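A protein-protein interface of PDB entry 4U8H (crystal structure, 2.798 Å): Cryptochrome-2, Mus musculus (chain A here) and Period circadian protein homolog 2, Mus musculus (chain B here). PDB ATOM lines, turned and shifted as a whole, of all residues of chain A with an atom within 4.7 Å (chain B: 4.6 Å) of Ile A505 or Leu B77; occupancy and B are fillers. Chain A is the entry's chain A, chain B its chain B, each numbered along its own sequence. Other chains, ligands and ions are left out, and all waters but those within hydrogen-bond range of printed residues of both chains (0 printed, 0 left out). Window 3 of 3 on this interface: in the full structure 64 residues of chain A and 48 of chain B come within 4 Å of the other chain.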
ATOM      1  N   ILE A 334      12.323   5.160  -8.551  1.00  0.00           N
ATOM      2  CA  ILE A 334      13.187   4.741  -7.459  1.00  0.00           C
ATOM      3  C   ILE A 334      14.587   5.257  -7.705  1.00  0.00           C
ATOM      4  O   ILE A 334      15.092   5.154  -8.820  1.00  0.00           O
ATOM      5  CB  ILE A 334      13.222   3.184  -7.360  1.00  0.00           C
ATOM      6  CG1 ILE A 334      11.837   2.641  -7.030  1.00  0.00           C
ATOM      7  CG2 ILE A 334      14.185   2.693  -6.321  1.00  0.00           C
ATOM      8  CD1 ILE A 334      11.010   3.534  -6.141  1.00  0.00           C
ATOM      9  N   GLN A 335      15.200   5.838  -6.675  1.00  0.00           N
ATOM     10  CA  GLN A 335      16.592   6.266  -6.758  1.00  0.00           C
ATOM     11  C   GLN A 335      17.481   5.146  -6.218  1.00  0.00           C
ATOM     12  O   GLN A 335      17.197   4.542  -5.185  1.00  0.00           O
ATOM     13  CB  GLN A 335      16.816   7.575  -5.994  1.00  0.00           C
ATOM     14  CG  GLN A 335      15.610   8.487  -5.992  1.00  0.00           C
ATOM     15  CD  GLN A 335      15.467   9.304  -7.258  1.00  0.00           C
ATOM     16  OE1 GLN A 335      16.427   9.486  -8.000  1.00  0.00           O
ATOM     17  NE2 GLN A 335      14.262   9.815  -7.505  1.00  0.00           N
ATOM     18  N   ILE A 336      18.566   4.874  -6.926  1.00  0.00           N
ATOM     19  CA  ILE A 336      19.331   3.654  -6.710  1.00  0.00           C
ATOM     20  C   ILE A 336      20.796   3.955  -6.956  1.00  0.00           C
ATOM     21  O   ILE A 336      21.129   4.675  -7.897  1.00  0.00           O
ATOM     22  CB  ILE A 336      18.858   2.541  -7.692  1.00  0.00           C
ATOM     23  CG1 ILE A 336      17.480   2.015  -7.295  1.00  0.00           C
ATOM     24  CG2 ILE A 336      19.855   1.385  -7.774  1.00  0.00           C
ATOM     25  CD1 ILE A 336      16.973   0.938  -8.195  1.00  0.00           C
ATOM     26  N   PRO A 337      21.677   3.407  -6.109  1.00  0.00           N
ATOM     27  CA  PRO A 337      23.119   3.655  -6.229  1.00  0.00           C
ATOM     28  C   PRO A 337      23.783   2.855  -7.345  1.00  0.00           C
ATOM     29  O   PRO A 337      24.604   1.983  -7.066  1.00  0.00           O
ATOM     30  CB  PRO A 337      23.660   3.215  -4.865  1.00  0.00           C
ATOM     31  CG  PRO A 337      22.694   2.174  -4.403  1.00  0.00           C
ATOM     32  CD  PRO A 337      21.347   2.600  -4.918  1.00  0.00           C
ATOM     33  N   TRP A 389      25.168  -3.492 -12.873  1.00  0.00           N
ATOM     34  CA  TRP A 389      24.700  -2.380 -12.067  1.00  0.00           C
ATOM     35  C   TRP A 389      24.957  -0.984 -12.673  1.00  0.00           C
ATOM     36  O   TRP A 389      25.303  -0.058 -11.942  1.00  0.00           O
ATOM     37  CB  TRP A 389      25.286  -2.473 -10.646  1.00  0.00           C
ATOM     38  CG  TRP A 389      24.341  -1.963  -9.593  1.00  0.00           C
ATOM     39  CD1 TRP A 389      24.329  -0.724  -9.036  1.00  0.00           C
ATOM     40  CD2 TRP A 389      23.248  -2.677  -9.003  1.00  0.00           C
ATOM     41  NE1 TRP A 389      23.302  -0.617  -8.134  1.00  0.00           N
ATOM     42  CE2 TRP A 389      22.624  -1.805  -8.094  1.00  0.00           C
ATOM     43  CE3 TRP A 389      22.744  -3.974  -9.149  1.00  0.00           C
ATOM     44  CZ2 TRP A 389      21.527  -2.183  -7.337  1.00  0.00           C
ATOM     45  CZ3 TRP A 389      21.655  -4.346  -8.403  1.00  0.00           C
ATOM     46  CH2 TRP A 389      21.055  -3.454  -7.508  1.00  0.00           C
ATOM     47  N   ARG A 501      22.063  -6.598  -2.969  1.00  0.00           N
ATOM     48  CA  ARG A 501      22.036  -5.137  -3.085  1.00  0.00           C
ATOM     49  C   ARG A 501      20.653  -4.690  -3.505  1.00  0.00           C
ATOM     50  O   ARG A 501      20.180  -3.617  -3.127  1.00  0.00           O
ATOM     51  CB  ARG A 501      23.049  -4.646  -4.121  1.00  0.00           C
ATOM     52  CG  ARG A 501      24.490  -5.026  -3.838  1.00  0.00           C
ATOM     53  CD  ARG A 501      25.371  -4.716  -5.037  1.00  0.00           C
ATOM     54  NE  ARG A 501      25.438  -3.284  -5.297  1.00  0.00           N
ATOM     55  CZ  ARG A 501      26.226  -2.723  -6.211  1.00  0.00           C
ATOM     56  NH1 ARG A 501      27.024  -3.475  -6.971  1.00  0.00           N
ATOM     57  NH2 ARG A 501      26.215  -1.403  -6.359  1.00  0.00           N
ATOM     58  N   MET A 502      19.999  -5.522  -4.300  1.00  0.00           N
ATOM     59  CA  MET A 502      18.650  -5.199  -4.720  1.00  0.00           C
ATOM     60  C   MET A 502      17.685  -5.317  -3.550  1.00  0.00           C
ATOM     61  O   MET A 502      16.848  -4.432  -3.345  1.00  0.00           O
ATOM     62  CB  MET A 502      18.190  -6.071  -5.887  1.00  0.00           C
ATOM     63  CG  MET A 502      17.047  -5.433  -6.650  1.00  0.00           C
ATOM     64  SD  MET A 502      17.620  -3.968  -7.518  1.00  0.00           S
ATOM     65  CE  MET A 502      16.122  -2.990  -7.565  1.00  0.00           C
ATOM     66  N   LYS A 503      17.805  -6.401  -2.783  1.00  0.00           N
ATOM     67  CA  LYS A 503      16.966  -6.564  -1.598  1.00  0.00           C
ATOM     68  C   LYS A 503      17.207  -5.419  -0.620  1.00  0.00           C
ATOM     69  O   LYS A 503      16.262  -4.868  -0.065  1.00  0.00           O
ATOM     70  CB  LYS A 503      17.190  -7.921  -0.917  1.00  0.00           C
ATOM     71  CG  LYS A 503      16.483  -9.086  -1.613  1.00  0.00           C
ATOM     72  CD  LYS A 503      16.507 -10.352  -0.771  1.00  0.00           C
ATOM     73  CE  LYS A 503      17.920 -10.678  -0.302  1.00  0.00           C
ATOM     74  NZ  LYS A 503      18.751 -11.448  -1.266  1.00  0.00           N
ATOM     75  N   GLN A 504      18.469  -5.043  -0.440  1.00  0.00           N
ATOM     76  CA  GLN A 504      18.812  -3.937   0.443  1.00  0.00           C
ATOM     77  C   GLN A 504      18.091  -2.620   0.127  1.00  0.00           C
ATOM     78  O   GLN A 504      17.637  -1.920   1.025  1.00  0.00           O
ATOM     79  CB  GLN A 504      20.316  -3.720   0.451  1.00  0.00           C
ATOM     80  CG  GLN A 504      20.769  -2.788   1.536  1.00  0.00           C
ATOM     81  CD  GLN A 504      22.270  -2.779   1.665  1.00  0.00           C
ATOM     82  OE1 GLN A 504      22.807  -2.739   2.770  1.00  0.00           O
ATOM     83  NE2 GLN A 504      22.962  -2.802   0.529  1.00  0.00           N
ATOM     84  N   ILE A 505      17.985  -2.291  -1.152  1.00  0.00           N
ATOM     85  CA  ILE A 505      17.316  -1.066  -1.569  1.00  0.00           C
ATOM     86  C   ILE A 505      15.835  -1.156  -1.223  1.00  0.00           C
ATOM     87  O   ILE A 505      15.169  -0.141  -0.964  1.00  0.00           O
ATOM     88  CB  ILE A 505      17.517  -0.835  -3.073  1.00  0.00           C
ATOM     89  CG1 ILE A 505      18.999  -0.611  -3.359  1.00  0.00           C
ATOM     90  CG2 ILE A 505      16.691   0.349  -3.582  1.00  0.00           C
ATOM     91  CD1 ILE A 505      19.364  -0.779  -4.807  1.00  0.00           C
ATOM     92  N   TYR A 506      15.349  -2.398  -1.202  1.00  0.00           N
ATOM     93  CA  TYR A 506      13.945  -2.708  -0.963  1.00  0.00           C
ATOM     94  C   TYR A 506      13.622  -2.942   0.507  1.00  0.00           C
ATOM     95  O   TYR A 506      12.571  -2.511   0.977  1.00  0.00           O
ATOM     96  CB  TYR A 506      13.503  -3.882  -1.844  1.00  0.00           C
ATOM     97  CG  TYR A 506      13.060  -3.391  -3.195  1.00  0.00           C
ATOM     98  CD1 TYR A 506      11.772  -2.900  -3.381  1.00  0.00           C
ATOM     99  CD2 TYR A 506      13.941  -3.355  -4.274  1.00  0.00           C
ATOM    100  CE1 TYR A 506      11.363  -2.409  -4.604  1.00  0.00           C
ATOM    101  CE2 TYR A 506      13.535  -2.868  -5.502  1.00  0.00           C
ATOM    102  CZ  TYR A 506      12.249  -2.399  -5.658  1.00  0.00           C
ATOM    103  OH  TYR A 506      11.841  -1.912  -6.869  1.00  0.00           O
ATOM    104  N   GLN A 507      14.521  -3.618   1.221  1.00  0.00           N
ATOM    105  CA  GLN A 507      14.437  -3.712   2.675  1.00  0.00           C
ATOM    106  C   GLN A 507      14.331  -2.296   3.191  1.00  0.00           C
ATOM    107  O   GLN A 507      13.294  -1.884   3.701  1.00  0.00           O
ATOM    108  CB  GLN A 507      15.700  -4.350   3.264  1.00  0.00           C
ATOM    109  CG  GLN A 507      15.818  -5.861   3.111  1.00  0.00           C
ATOM    110  CD  GLN A 507      17.261  -6.338   3.224  1.00  0.00           C
ATOM    111  OE1 GLN A 507      18.166  -5.562   3.565  1.00  0.00           O
ATOM    112  NE2 GLN A 507      17.485  -7.617   2.926  1.00  0.00           N
ATOM    113  N   GLN A 508      15.418  -1.550   3.024  1.00  0.00           N
ATOM    114  CA  GLN A 508      15.482  -0.144   3.409  1.00  0.00           C
ATOM    115  C   GLN A 508      14.766   0.735   2.392  1.00  0.00           C
ATOM    116  O   GLN A 508      15.404   1.498   1.659  1.00  0.00           O
ATOM    117  CB  GLN A 508      16.942   0.304   3.551  1.00  0.00           C
ATOM    118  CG  GLN A 508      17.749  -0.508   4.558  1.00  0.00           C
ATOM    119  CD  GLN A 508      17.070  -0.604   5.914  1.00  0.00           C
ATOM    120  OE1 GLN A 508      16.474  -1.627   6.245  1.00  0.00           O
ATOM    121  NE2 GLN A 508      17.160   0.461   6.706  1.00  0.00           N
ATOM    122  N   LEU A 509      13.442   0.619   2.366  1.00  0.00           N
ATOM    123  CA  LEU A 509      12.596   1.345   1.432  1.00  0.00           C
ATOM    124  C   LEU A 509      11.231   1.525   2.068  1.00  0.00           C
ATOM    125  O   LEU A 509      10.574   0.544   2.445  1.00  0.00           O
ATOM    126  CB  LEU A 509      12.449   0.567   0.126  1.00  0.00           C
ATOM    127  CG  LEU A 509      11.768   1.257  -1.060  1.00  0.00           C
ATOM    128  CD1 LEU A 509      12.666   2.295  -1.664  1.00  0.00           C
ATOM    129  CD2 LEU A 509      11.397   0.232  -2.102  1.00  0.00           C
ATOM    130  N   ASP B  73      26.091   1.366  -0.280  1.00  0.00           N
ATOM    131  CA  ASP B  73      24.747   1.616  -0.775  1.00  0.00           C
ATOM    132  C   ASP B  73      23.874   2.257   0.308  1.00  0.00           C
ATOM    133  O   ASP B  73      23.120   3.186   0.029  1.00  0.00           O
ATOM    134  CB  ASP B  73      24.112   0.321  -1.311  1.00  0.00           C
ATOM    135  CG  ASP B  73      24.610  -0.055  -2.715  1.00  0.00           C
ATOM    136  OD1 ASP B  73      25.727   0.361  -3.091  1.00  0.00           O
ATOM    137  OD2 ASP B  73      23.885  -0.775  -3.445  1.00  0.00           O
ATOM    138  N   GLN B  74      23.999   1.769   1.541  1.00  0.00           N
ATOM    139  CA  GLN B  74      23.240   2.293   2.677  1.00  0.00           C
ATOM    140  C   GLN B  74      23.439   3.794   2.844  1.00  0.00           C
ATOM    141  O   GLN B  74      22.477   4.541   3.051  1.00  0.00           O
ATOM    142  CB  GLN B  74      23.652   1.588   3.972  1.00  0.00           C
ATOM    143  CG  GLN B  74      23.497   0.078   3.943  1.00  0.00           C
ATOM    144  CD  GLN B  74      23.980  -0.596   5.223  1.00  0.00           C
ATOM    145  OE1 GLN B  74      24.927  -0.136   5.865  1.00  0.00           O
ATOM    146  NE2 GLN B  74      23.321  -1.690   5.599  1.00  0.00           N
ATOM    147  N   GLU B  75      24.692   4.225   2.750  1.00  0.00           N
ATOM    148  CA  GLU B  75      25.040   5.626   2.943  1.00  0.00           C
ATOM    149  C   GLU B  75      24.515   6.505   1.825  1.00  0.00           C
ATOM    150  O   GLU B  75      23.893   7.538   2.076  1.00  0.00           O
ATOM    151  CB  GLU B  75      26.546   5.779   3.045  1.00  0.00           C
ATOM    152  CG  GLU B  75      27.116   5.159   4.287  1.00  0.00           C
ATOM    153  CD  GLU B  75      28.608   4.984   4.196  1.00  0.00           C
ATOM    154  OE1 GLU B  75      29.229   5.614   3.319  1.00  0.00           O
ATOM    155  OE2 GLU B  75      29.163   4.204   4.994  1.00  0.00           O
ATOM    156  N   LYS B  76      24.778   6.090   0.591  1.00  0.00           N
ATOM    157  CA  LYS B  76      24.240   6.786  -0.567  1.00  0.00           C
ATOM    158  C   LYS B  76      22.724   6.824  -0.482  1.00  0.00           C
ATOM    159  O   LYS B  76      22.108   7.828  -0.819  1.00  0.00           O
ATOM    160  CB  LYS B  76      24.667   6.106  -1.863  1.00  0.00           C
ATOM    161  CG  LYS B  76      26.146   6.220  -2.176  1.00  0.00           C
ATOM    162  CD  LYS B  76      26.458   5.676  -3.561  1.00  0.00           C
ATOM    163  CE  LYS B  76      27.910   5.264  -3.686  1.00  0.00           C
ATOM    164  NZ  LYS B  76      28.244   4.941  -5.096  1.00  0.00           N
ATOM    165  N   LEU B  77      22.127   5.731  -0.019  1.00  0.00           N
ATOM    166  CA  LEU B  77      20.677   5.653   0.082  1.00  0.00           C
ATOM    167  C   LEU B  77      20.154   6.678   1.074  1.00  0.00           C
ATOM    168  O   LEU B  77      19.082   7.262   0.883  1.00  0.00           O
ATOM    169  CB  LEU B  77      20.244   4.243   0.471  1.00  0.00           C
ATOM    170  CG  LEU B  77      20.026   3.350  -0.747  1.00  0.00           C
ATOM    171  CD1 LEU B  77      19.758   1.896  -0.355  1.00  0.00           C
ATOM    172  CD2 LEU B  77      18.879   3.913  -1.575  1.00  0.00           C
ATOM    173  N   LYS B  78      20.927   6.911   2.128  1.00  0.00           N
ATOM    174  CA  LYS B  78      20.501   7.855   3.144  1.00  0.00           C
ATOM    175  C   LYS B  78      20.461   9.244   2.535  1.00  0.00           C
ATOM    176  O   LYS B  78      19.558  10.024   2.834  1.00  0.00           O
ATOM    177  CB  LYS B  78      21.379   7.772   4.396  1.00  0.00           C
ATOM    178  CG  LYS B  78      21.132   6.504   5.214  1.00  0.00           C
ATOM    179  CD  LYS B  78      21.735   6.566   6.610  1.00  0.00           C
ATOM    180  CE  LYS B  78      21.490   5.254   7.354  1.00  0.00           C
ATOM    181  NZ  LYS B  78      21.914   5.295   8.784  1.00  0.00           N
ATOM    182  N   LEU B  79      21.424   9.531   1.657  1.00  0.00           N
ATOM    183  CA  LEU B  79      21.366  10.722   0.801  1.00  0.00           C
ATOM    184  C   LEU B  79      20.122  10.672  -0.066  1.00  0.00           C
ATOM    185  O   LEU B  79      19.256  11.548   0.001  1.00  0.00           O
ATOM    186  CB  LEU B  79      22.569  10.790  -0.158  1.00  0.00           C
ATOM    187  CG  LEU B  79      23.966  11.282   0.230  1.00  0.00           C
ATOM    188  CD1 LEU B  79      24.870  11.340  -0.994  1.00  0.00           C
ATOM    189  CD2 LEU B  79      23.889  12.641   0.887  1.00  0.00           C
ATOM    190  N   LEU B  80      20.067   9.624  -0.884  1.00  0.00           N
ATOM    191  CA  LEU B  80      19.081   9.476  -1.938  1.00  0.00           C
ATOM    192  C   LEU B  80      17.682   9.513  -1.392  1.00  0.00           C
ATOM    193  O   LEU B  80      16.824  10.203  -1.949  1.00  0.00           O
ATOM    194  CB  LEU B  80      19.297   8.159  -2.683  1.00  0.00           C
ATOM    195  CG  LEU B  80      20.582   8.043  -3.495  1.00  0.00           C
ATOM    196  CD1 LEU B  80      21.022   6.598  -3.624  1.00  0.00           C
ATOM    197  CD2 LEU B  80      20.391   8.665  -4.862  1.00  0.00           C
ATOM    198  N   GLN B  81      17.454   8.787  -0.296  1.00  0.00           N
ATOM    199  CA  GLN B  81      16.098   8.584   0.213  1.00  0.00           C
ATOM    200  C   GLN B  81      15.455   9.894   0.667  1.00  0.00           C
ATOM    201  O   GLN B  81      14.908  10.003   1.756  1.00  0.00           O
ATOM    202  CB  GLN B  81      16.028   7.459   1.273  1.00  0.00           C
ATOM    203  CG  GLN B  81      16.321   6.044   0.688  1.00  0.00           C
ATOM    204  CD  GLN B  81      15.758   4.885   1.518  1.00  0.00           C
ATOM    205  OE1 GLN B  81      14.830   5.068   2.311  1.00  0.00           O
ATOM    206  NE2 GLN B  81      16.321   3.685   1.327  1.00  0.00           N
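NE of Arg A501 lies within salt-bridge range of OD2 of Asp B73 (3.5 Å). The side-chain amide nitrogen (NE2) of Gln B74 lies within hydrogen-bond range of the side-chain amide oxygen (OE1) of Gln A504 (3.1 Å). The side-chain amide nitrogen of Gln B81 sits close to the backbone carbonyl oxygen of Gln A508, at 2.4 Å.
NE1 of Trp A389 sits at hydrogen-bond distance from O of Pro A337 (3.1 Å).
Gln A335 touches Leu B80. OD2 of Asp B73 touches CG of Pro A337, at 3.3 Å. CB of Pro A337 touches CD of Lys B76, at 3.9 Å. CB of Asp B73 touches NE2 of Gln A504, at 3.8 Å. Leu B77 touches Ile A505.
Of the printed residues of chain B, Ile A505 touches Leu B77 (3.99 Å). Of the printed residues of chain A, Leu B77 touches Ile A505. Printed residues of chain A within 4 Å of Lys B76: Pro A337 (3.9 Å). Printed residues of chain A within 4 Å of Gln B81: Gln A508. Of the printed residues of chain A, Leu B80 touches Gln A335.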
